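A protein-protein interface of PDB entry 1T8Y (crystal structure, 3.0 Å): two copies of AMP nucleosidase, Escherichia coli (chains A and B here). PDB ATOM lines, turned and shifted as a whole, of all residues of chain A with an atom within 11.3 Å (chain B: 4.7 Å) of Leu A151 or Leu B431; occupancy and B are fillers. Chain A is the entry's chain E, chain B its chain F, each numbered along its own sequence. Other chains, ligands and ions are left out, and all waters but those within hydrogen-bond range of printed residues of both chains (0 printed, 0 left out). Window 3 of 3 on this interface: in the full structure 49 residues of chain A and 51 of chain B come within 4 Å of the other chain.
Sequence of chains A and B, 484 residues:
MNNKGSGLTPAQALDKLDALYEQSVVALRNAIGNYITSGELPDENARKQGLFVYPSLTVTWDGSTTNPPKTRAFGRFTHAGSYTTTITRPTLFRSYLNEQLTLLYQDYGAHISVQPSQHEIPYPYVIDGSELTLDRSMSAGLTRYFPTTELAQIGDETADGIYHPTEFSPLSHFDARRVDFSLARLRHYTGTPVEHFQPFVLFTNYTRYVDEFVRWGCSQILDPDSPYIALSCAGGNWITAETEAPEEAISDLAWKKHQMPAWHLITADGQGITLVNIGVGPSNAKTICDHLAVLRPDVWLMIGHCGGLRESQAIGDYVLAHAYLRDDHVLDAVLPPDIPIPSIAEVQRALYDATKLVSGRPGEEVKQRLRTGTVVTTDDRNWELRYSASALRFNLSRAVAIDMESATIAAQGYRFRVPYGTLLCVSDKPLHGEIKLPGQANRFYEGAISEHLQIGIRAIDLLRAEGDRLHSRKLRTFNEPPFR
No position is printed for both chains.
Printed residues of chain B that touch a printed residue of chain A: Glu B384, Pro B430, Leu B431, Gly B433 and Ile B435.
Hydrophobic or aromatic side chains of chain B within 4 Å of the printed part of chain A: Ile B435.
Among the printed residues, 7 pairs touch across the chains.
Among the printed residues, no Asp or Glu carboxylate lies within 4 Å of a Lys or Arg side-chain nitrogen of the other chain.
Thr A143 touches none of the printed residues of chain B.
Of the printed residues of chain B, Thr A149 touches Gly B433 and Ile B435.
Of chain B, only Glu B384 (3.7 Å), Pro B430 (3.1 Å), Leu B431 (3.7 Å) and Ile B435 (3.9 Å) come within 4 Å of Leu A151.
Of the printed residues of chain B, Arg A185 touches Ile B435.
No residue of chain A comes within 4 Å of Leu B309.
No residue of chain A comes within 4 Å of Lys B429.
Pro B430 touches one residue of chain A.
Of chain A, only Leu A151 (3.7 Å) comes within 4 Å of Leu B431.
No residue of chain A comes within 4 Å of His B432.
Of chain A, only Thr A149 (3.3 Å) comes within 4 Å of Gly B433.
Printed residues of chain A within 4 Å of Ile B435: Thr A149 (3.9 Å), Leu A151 (3.9 Å) and Arg A185 (2.9 Å).
The nearest printed residue of chain B that does not touch Arg A185 is Glu B384 (4.7 Å).
Among the printed residues, merely in contact across the chains: Leu A151 with Pro B430 (3.1 Å), Leu A151 with Glu B384 (3.7 Å), Leu A151 with Leu B431 (3.7 Å), Leu A151 with Ile B435 (3.9 Å) and Thr A149 with Ile B435 (3.9 Å).
The backbone carbonyl oxygen (O) of Gly B433 lies within hydrogen-bond range of the side-chain hydroxyl (OG1) of Thr A149 (3.3 Å).
NH2 of Arg A185 lies close to O of Ile B435 (3.1 Å).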
ATOM      1  N   HIS A 119      23.668  27.698  20.266  1.00  0.00           N
ATOM      2  CA  HIS A 119      22.252  28.005  20.381  1.00  0.00           C
ATOM      3  C   HIS A 119      21.946  29.471  20.600  1.00  0.00           C
ATOM      4  O   HIS A 119      22.419  30.087  21.559  1.00  0.00           O
ATOM      5  CB  HIS A 119      21.664  27.177  21.512  1.00  0.00           C
ATOM      6  CG  HIS A 119      21.924  25.713  21.367  1.00  0.00           C
ATOM      7  ND1 HIS A 119      21.199  24.910  20.510  1.00  0.00           N
ATOM      8  CD2 HIS A 119      22.875  24.920  21.916  1.00  0.00           C
ATOM      9  CE1 HIS A 119      21.695  23.685  20.538  1.00  0.00           C
ATOM     10  NE2 HIS A 119      22.713  23.664  21.382  1.00  0.00           N
ATOM     11  N   GLU A 120      21.142  30.023  19.701  1.00  0.00           N
ATOM     12  CA  GLU A 120      20.753  31.419  19.801  1.00  0.00           C
ATOM     13  C   GLU A 120      19.618  31.577  20.806  1.00  0.00           C
ATOM     14  O   GLU A 120      18.869  30.634  21.081  1.00  0.00           O
ATOM     15  CB  GLU A 120      20.314  31.951  18.432  1.00  0.00           C
ATOM     16  CG  GLU A 120      21.392  31.807  17.358  1.00  0.00           C
ATOM     17  CD  GLU A 120      21.035  32.506  16.050  1.00  0.00           C
ATOM     18  OE1 GLU A 120      20.007  32.135  15.434  1.00  0.00           O
ATOM     19  OE2 GLU A 120      21.791  33.426  15.644  1.00  0.00           O
ATOM     20  N   PRO A 122      16.080  32.759  21.795  1.00  0.00           N
ATOM     21  CA  PRO A 122      14.835  33.108  21.094  1.00  0.00           C
ATOM     22  C   PRO A 122      14.544  34.577  21.398  1.00  0.00           C
ATOM     23  O   PRO A 122      14.657  35.007  22.553  1.00  0.00           O
ATOM     24  CB  PRO A 122      13.815  32.162  21.717  1.00  0.00           C
ATOM     25  CG  PRO A 122      14.653  30.941  22.015  1.00  0.00           C
ATOM     26  CD  PRO A 122      15.904  31.550  22.619  1.00  0.00           C
ATOM     27  N   TYR A 125      12.657  36.086  24.656  1.00  0.00           N
ATOM     28  CA  TYR A 125      13.336  36.132  25.942  1.00  0.00           C
ATOM     29  C   TYR A 125      14.223  37.363  26.164  1.00  0.00           C
ATOM     30  O   TYR A 125      14.690  37.588  27.278  1.00  0.00           O
ATOM     31  CB  TYR A 125      14.180  34.861  26.151  1.00  0.00           C
ATOM     32  CG  TYR A 125      13.381  33.577  26.141  1.00  0.00           C
ATOM     33  CD1 TYR A 125      12.238  33.433  26.928  1.00  0.00           C
ATOM     34  CD2 TYR A 125      13.770  32.506  25.352  1.00  0.00           C
ATOM     35  CE1 TYR A 125      11.503  32.246  26.928  1.00  0.00           C
ATOM     36  CE2 TYR A 125      13.043  31.316  25.341  1.00  0.00           C
ATOM     37  CZ  TYR A 125      11.912  31.191  26.131  1.00  0.00           C
ATOM     38  OH  TYR A 125      11.197  30.013  26.118  1.00  0.00           O
ATOM     39  N   THR A 143       9.471  36.309  13.400  1.00  0.00           N
ATOM     40  CA  THR A 143       9.596  34.858  13.565  1.00  0.00           C
ATOM     41  C   THR A 143      10.294  34.169  12.382  1.00  0.00           C
ATOM     42  O   THR A 143      10.719  33.016  12.494  1.00  0.00           O
ATOM     43  CB  THR A 143       8.204  34.192  13.808  1.00  0.00           C
ATOM     44  OG1 THR A 143       7.353  34.405  12.674  1.00  0.00           O
ATOM     45  CG2 THR A 143       7.541  34.779  15.059  1.00  0.00           C
ATOM     46  N   PRO A 147      15.821  34.346  15.908  1.00  0.00           N
ATOM     47  CA  PRO A 147      15.799  33.164  16.770  1.00  0.00           C
ATOM     48  C   PRO A 147      14.464  33.012  17.487  1.00  0.00           C
ATOM     49  O   PRO A 147      14.098  33.853  18.320  1.00  0.00           O
ATOM     50  CB  PRO A 147      16.945  33.425  17.747  1.00  0.00           C
ATOM     51  CG  PRO A 147      17.890  34.228  16.938  1.00  0.00           C
ATOM     52  CD  PRO A 147      16.969  35.203  16.246  1.00  0.00           C
ATOM     53  N   THR A 148      13.740  31.944  17.152  1.00  0.00           N
ATOM     54  CA  THR A 148      12.448  31.663  17.773  1.00  0.00           C
ATOM     55  C   THR A 148      12.509  30.352  18.558  1.00  0.00           C
ATOM     56  O   THR A 148      13.518  29.636  18.532  1.00  0.00           O
ATOM     57  CB  THR A 148      11.306  31.549  16.731  1.00  0.00           C
ATOM     58  OG1 THR A 148      11.479  30.354  15.959  1.00  0.00           O
ATOM     59  CG2 THR A 148      11.303  32.761  15.803  1.00  0.00           C
ATOM     60  N   THR A 149      11.415  30.044  19.249  1.00  0.00           N
ATOM     61  CA  THR A 149      11.342  28.835  20.056  1.00  0.00           C
ATOM     62  C   THR A 149      11.039  27.603  19.221  1.00  0.00           C
ATOM     63  O   THR A 149       9.960  27.470  18.634  1.00  0.00           O
ATOM     64  CB  THR A 149      10.270  28.956  21.150  1.00  0.00           C
ATOM     65  OG1 THR A 149      10.013  30.341  21.413  1.00  0.00           O
ATOM     66  CG2 THR A 149      10.752  28.291  22.437  1.00  0.00           C
ATOM     67  N   GLU A 150      12.024  26.713  19.173  1.00  0.00           N
ATOM     68  CA  GLU A 150      11.917  25.456  18.445  1.00  0.00           C
ATOM     69  C   GLU A 150      11.723  24.384  19.517  1.00  0.00           C
ATOM     70  O   GLU A 150      12.486  24.339  20.489  1.00  0.00           O
ATOM     71  CB  GLU A 150      13.215  25.167  17.687  1.00  0.00           C
ATOM     72  CG  GLU A 150      13.731  26.301  16.814  1.00  0.00           C
ATOM     73  CD  GLU A 150      15.246  26.239  16.634  1.00  0.00           C
ATOM     74  OE1 GLU A 150      15.963  26.437  17.641  1.00  0.00           O
ATOM     75  OE2 GLU A 150      15.719  25.988  15.499  1.00  0.00           O
ATOM     76  N   LEU A 151      10.712  23.532  19.345  1.00  0.00           N
ATOM     77  CA  LEU A 151      10.426  22.469  20.311  1.00  0.00           C
ATOM     78  C   LEU A 151      11.445  21.336  20.213  1.00  0.00           C
ATOM     79  O   LEU A 151      12.181  21.059  21.164  1.00  0.00           O
ATOM     80  CB  LEU A 151       9.016  21.907  20.088  1.00  0.00           C
ATOM     81  CG  LEU A 151       7.818  22.857  20.175  1.00  0.00           C
ATOM     82  CD1 LEU A 151       7.844  23.600  21.502  1.00  0.00           C
ATOM     83  CD2 LEU A 151       7.849  23.833  19.000  1.00  0.00           C
ATOM     84  N   ASP A 175      18.944  23.037  30.397  1.00  0.00           N
ATOM     85  CA  ASP A 175      19.797  23.850  29.544  1.00  0.00           C
ATOM     86  C   ASP A 175      19.183  25.257  29.406  1.00  0.00           C
ATOM     87  O   ASP A 175      18.035  25.494  29.811  1.00  0.00           O
ATOM     88  CB  ASP A 175      19.976  23.187  28.169  1.00  0.00           C
ATOM     89  CG  ASP A 175      18.771  23.372  27.266  1.00  0.00           C
ATOM     90  OD1 ASP A 175      17.685  22.840  27.597  1.00  0.00           O
ATOM     91  OD2 ASP A 175      18.921  24.062  26.224  1.00  0.00           O
ATOM     92  N   ARG A 177      17.710  27.210  27.100  1.00  0.00           N
ATOM     93  CA  ARG A 177      16.355  27.401  26.602  1.00  0.00           C
ATOM     94  C   ARG A 177      15.274  26.947  27.581  1.00  0.00           C
ATOM     95  O   ARG A 177      14.260  27.641  27.780  1.00  0.00           O
ATOM     96  CB  ARG A 177      16.162  26.665  25.284  1.00  0.00           C
ATOM     97  CG  ARG A 177      16.559  27.446  24.064  1.00  0.00           C
ATOM     98  CD  ARG A 177      15.681  27.056  22.868  1.00  0.00           C
ATOM     99  NE  ARG A 177      16.232  27.552  21.607  1.00  0.00           N
ATOM    100  CZ  ARG A 177      17.428  27.206  21.129  1.00  0.00           C
ATOM    101  NH1 ARG A 177      18.200  26.354  21.808  1.00  0.00           N
ATOM    102  NH2 ARG A 177      17.865  27.718  19.978  1.00  0.00           N
ATOM    103  N   ARG A 178      15.487  25.770  28.169  1.00  0.00           N
ATOM    104  CA  ARG A 178      14.545  25.201  29.128  1.00  0.00           C
ATOM    105  C   ARG A 178      14.362  26.157  30.289  1.00  0.00           C
ATOM    106  O   ARG A 178      13.241  26.422  30.706  1.00  0.00           O
ATOM    107  CB  ARG A 178      15.054  23.839  29.639  1.00  0.00           C
ATOM    108  CG  ARG A 178      14.193  23.171  30.719  1.00  0.00           C
ATOM    109  CD  ARG A 178      12.713  23.056  30.324  1.00  0.00           C
ATOM    110  NE  ARG A 178      11.880  23.024  31.524  1.00  0.00           N
ATOM    111  CZ  ARG A 178      11.568  21.920  32.194  1.00  0.00           C
ATOM    112  NH1 ARG A 178      12.004  20.732  31.774  1.00  0.00           N
ATOM    113  NH2 ARG A 178      10.864  22.008  33.312  1.00  0.00           N
ATOM    114  N   PHE A 181      12.515  29.469  29.300  1.00  0.00           N
ATOM    115  CA  PHE A 181      11.116  29.083  29.127  1.00  0.00           C
ATOM    116  C   PHE A 181      10.368  29.072  30.466  1.00  0.00           C
ATOM    117  O   PHE A 181       9.292  29.655  30.601  1.00  0.00           O
ATOM    118  CB  PHE A 181      11.074  27.682  28.514  1.00  0.00           C
ATOM    119  CG  PHE A 181       9.693  27.082  28.441  1.00  0.00           C
ATOM    120  CD1 PHE A 181       8.837  27.390  27.381  1.00  0.00           C
ATOM    121  CD2 PHE A 181       9.255  26.200  29.426  1.00  0.00           C
ATOM    122  CE1 PHE A 181       7.563  26.829  27.297  1.00  0.00           C
ATOM    123  CE2 PHE A 181       7.980  25.634  29.354  1.00  0.00           C
ATOM    124  CZ  PHE A 181       7.131  25.951  28.282  1.00  0.00           C
ATOM    125  N   ARG A 185       7.476  31.775  32.452  1.00  0.00           N
ATOM    126  CA  ARG A 185       6.234  31.268  33.038  1.00  0.00           C
ATOM    127  C   ARG A 185       6.110  31.531  34.537  1.00  0.00           C
ATOM    128  O   ARG A 185       5.065  31.991  34.997  1.00  0.00           O
ATOM    129  CB  ARG A 185       6.110  29.764  32.795  1.00  0.00           C
ATOM    130  CG  ARG A 185       5.414  29.376  31.515  1.00  0.00           C
ATOM    131  CD  ARG A 185       6.245  29.698  30.314  1.00  0.00           C
ATOM    132  NE  ARG A 185       5.535  29.309  29.107  1.00  0.00           N
ATOM    133  CZ  ARG A 185       5.958  29.557  27.873  1.00  0.00           C
ATOM    134  NH1 ARG A 185       7.111  30.203  27.674  1.00  0.00           N
ATOM    135  NH2 ARG A 185       5.217  29.166  26.839  1.00  0.00           N
ATOM    136  N   LEU B 309      -2.159  24.328  15.828  1.00  0.00           N
ATOM    137  CA  LEU B 309      -1.126  23.355  15.525  1.00  0.00           C
ATOM    138  C   LEU B 309      -0.750  23.370  14.065  1.00  0.00           C
ATOM    139  O   LEU B 309       0.311  22.876  13.683  1.00  0.00           O
ATOM    140  CB  LEU B 309      -1.590  21.960  15.945  1.00  0.00           C
ATOM    141  CG  LEU B 309      -1.895  21.828  17.438  1.00  0.00           C
ATOM    142  CD1 LEU B 309      -2.515  20.486  17.701  1.00  0.00           C
ATOM    143  CD2 LEU B 309      -0.624  22.004  18.252  1.00  0.00           C
ATOM    144  N   TRP B 383       2.899  20.510  27.715  1.00  0.00           N
ATOM    145  CA  TRP B 383       3.009  19.405  26.778  1.00  0.00           C
ATOM    146  C   TRP B 383       4.105  19.631  25.750  1.00  0.00           C
ATOM    147  O   TRP B 383       4.676  18.677  25.214  1.00  0.00           O
ATOM    148  CB  TRP B 383       1.681  19.187  26.061  1.00  0.00           C
ATOM    149  CG  TRP B 383       1.265  20.349  25.298  1.00  0.00           C
ATOM    150  CD1 TRP B 383       0.443  21.349  25.712  1.00  0.00           C
ATOM    151  CD2 TRP B 383       1.658  20.668  23.967  1.00  0.00           C
ATOM    152  NE1 TRP B 383       0.289  22.280  24.709  1.00  0.00           N
ATOM    153  CE2 TRP B 383       1.026  21.882  23.625  1.00  0.00           C
ATOM    154  CE3 TRP B 383       2.476  20.043  23.024  1.00  0.00           C
ATOM    155  CZ2 TRP B 383       1.195  22.487  22.384  1.00  0.00           C
ATOM    156  CZ3 TRP B 383       2.643  20.641  21.791  1.00  0.00           C
ATOM    157  CH2 TRP B 383       2.003  21.850  21.480  1.00  0.00           C
ATOM    158  N   GLU B 384       4.395  20.891  25.461  1.00  0.00           N
ATOM    159  CA  GLU B 384       5.427  21.186  24.492  1.00  0.00           C
ATOM    160  C   GLU B 384       6.717  20.504  24.928  1.00  0.00           C
ATOM    161  O   GLU B 384       7.462  19.987  24.096  1.00  0.00           O
ATOM    162  CB  GLU B 384       5.634  22.696  24.369  1.00  0.00           C
ATOM    163  CG  GLU B 384       4.360  23.472  24.041  1.00  0.00           C
ATOM    164  CD  GLU B 384       3.692  24.070  25.280  1.00  0.00           C
ATOM    165  OE1 GLU B 384       3.640  23.382  26.322  1.00  0.00           O
ATOM    166  OE2 GLU B 384       3.210  25.225  25.211  1.00  0.00           O
ATOM    167  N   TYR B 387       6.812  17.378  23.041  1.00  0.00           N
ATOM    168  CA  TYR B 387       6.267  17.303  21.691  1.00  0.00           C
ATOM    169  C   TYR B 387       6.530  15.987  20.959  1.00  0.00           C
ATOM    170  O   TYR B 387       5.590  15.279  20.582  1.00  0.00           O
ATOM    171  CB  TYR B 387       6.755  18.459  20.810  1.00  0.00           C
ATOM    172  CG  TYR B 387       6.080  18.419  19.451  1.00  0.00           C
ATOM    173  CD1 TYR B 387       4.695  18.222  19.354  1.00  0.00           C
ATOM    174  CD2 TYR B 387       6.819  18.511  18.264  1.00  0.00           C
ATOM    175  CE1 TYR B 387       4.058  18.111  18.116  1.00  0.00           C
ATOM    176  CE2 TYR B 387       6.185  18.400  17.009  1.00  0.00           C
ATOM    177  CZ  TYR B 387       4.802  18.199  16.951  1.00  0.00           C
ATOM    178  OH  TYR B 387       4.143  18.091  15.746  1.00  0.00           O
ATOM    179  N   LYS B 429       0.657  29.834  18.577  1.00  0.00           N
ATOM    180  CA  LYS B 429       1.088  28.692  17.781  1.00  0.00           C
ATOM    181  C   LYS B 429       2.381  28.130  18.355  1.00  0.00           C
ATOM    182  O   LYS B 429       3.476  28.474  17.917  1.00  0.00           O
ATOM    183  CB  LYS B 429       1.263  29.145  16.336  1.00  0.00           C
ATOM    184  CG  LYS B 429      -0.008  29.781  15.787  1.00  0.00           C
ATOM    185  CD  LYS B 429       0.185  30.276  14.372  1.00  0.00           C
ATOM    186  CE  LYS B 429       0.450  29.131  13.413  1.00  0.00           C
ATOM    187  NZ  LYS B 429      -0.718  28.220  13.410  1.00  0.00           N
ATOM    188  N   PRO B 430       2.255  27.229  19.337  1.00  0.00           N
ATOM    189  CA  PRO B 430       3.376  26.587  20.030  1.00  0.00           C
ATOM    190  C   PRO B 430       4.399  25.941  19.107  1.00  0.00           C
ATOM    191  O   PRO B 430       5.606  25.981  19.368  1.00  0.00           O
ATOM    192  CB  PRO B 430       2.687  25.554  20.935  1.00  0.00           C
ATOM    193  CG  PRO B 430       1.267  26.047  21.058  1.00  0.00           C
ATOM    194  CD  PRO B 430       0.992  26.548  19.665  1.00  0.00           C
ATOM    195  N   LEU B 431       3.906  25.350  18.025  1.00  0.00           N
ATOM    196  CA  LEU B 431       4.757  24.657  17.073  1.00  0.00           C
ATOM    197  C   LEU B 431       5.513  25.575  16.111  1.00  0.00           C
ATOM    198  O   LEU B 431       6.369  25.118  15.337  1.00  0.00           O
ATOM    199  CB  LEU B 431       3.899  23.652  16.297  1.00  0.00           C
ATOM    200  CG  LEU B 431       3.742  22.255  16.917  1.00  0.00           C
ATOM    201  CD1 LEU B 431       3.813  22.297  18.439  1.00  0.00           C
ATOM    202  CD2 LEU B 431       2.433  21.672  16.438  1.00  0.00           C
ATOM    203  N   HIS B 432       5.208  26.871  16.182  1.00  0.00           N
ATOM    204  CA  HIS B 432       5.831  27.856  15.305  1.00  0.00           C
ATOM    205  C   HIS B 432       6.340  29.117  16.014  1.00  0.00           C
ATOM    206  O   HIS B 432       6.006  30.235  15.614  1.00  0.00           O
ATOM    207  CB  HIS B 432       4.840  28.222  14.201  1.00  0.00           C
ATOM    208  CG  HIS B 432       4.201  27.027  13.562  1.00  0.00           C
ATOM    209  ND1 HIS B 432       3.191  26.309  14.168  1.00  0.00           N
ATOM    210  CD2 HIS B 432       4.469  26.390  12.397  1.00  0.00           C
ATOM    211  CE1 HIS B 432       2.865  25.282  13.404  1.00  0.00           C
ATOM    212  NE2 HIS B 432       3.627  25.308  12.324  1.00  0.00           N
ATOM    213  N   GLY B 433       7.136  28.919  17.071  1.00  0.00           N
ATOM    214  CA  GLY B 433       7.722  30.023  17.824  1.00  0.00           C
ATOM    215  C   GLY B 433       6.830  30.816  18.769  1.00  0.00           C
ATOM    216  O   GLY B 433       7.199  31.060  19.917  1.00  0.00           O
ATOM    217  N   ILE B 435       4.834  30.967  21.270  1.00  0.00           N
ATOM    218  CA  ILE B 435       4.317  30.225  22.422  1.00  0.00           C
ATOM    219  C   ILE B 435       3.921  31.177  23.551  1.00  0.00           C
ATOM    220  O   ILE B 435       4.563  31.197  24.605  1.00  0.00           O
ATOM    221  CB  ILE B 435       5.366  29.237  22.984  1.00  0.00           C
ATOM    222  CG1 ILE B 435       5.861  28.295  21.882  1.00  0.00           C
ATOM    223  CG2 ILE B 435       4.749  28.426  24.111  1.00  0.00           C
ATOM    224  CD1 ILE B 435       6.913  27.291  22.344  1.00  0.00           C
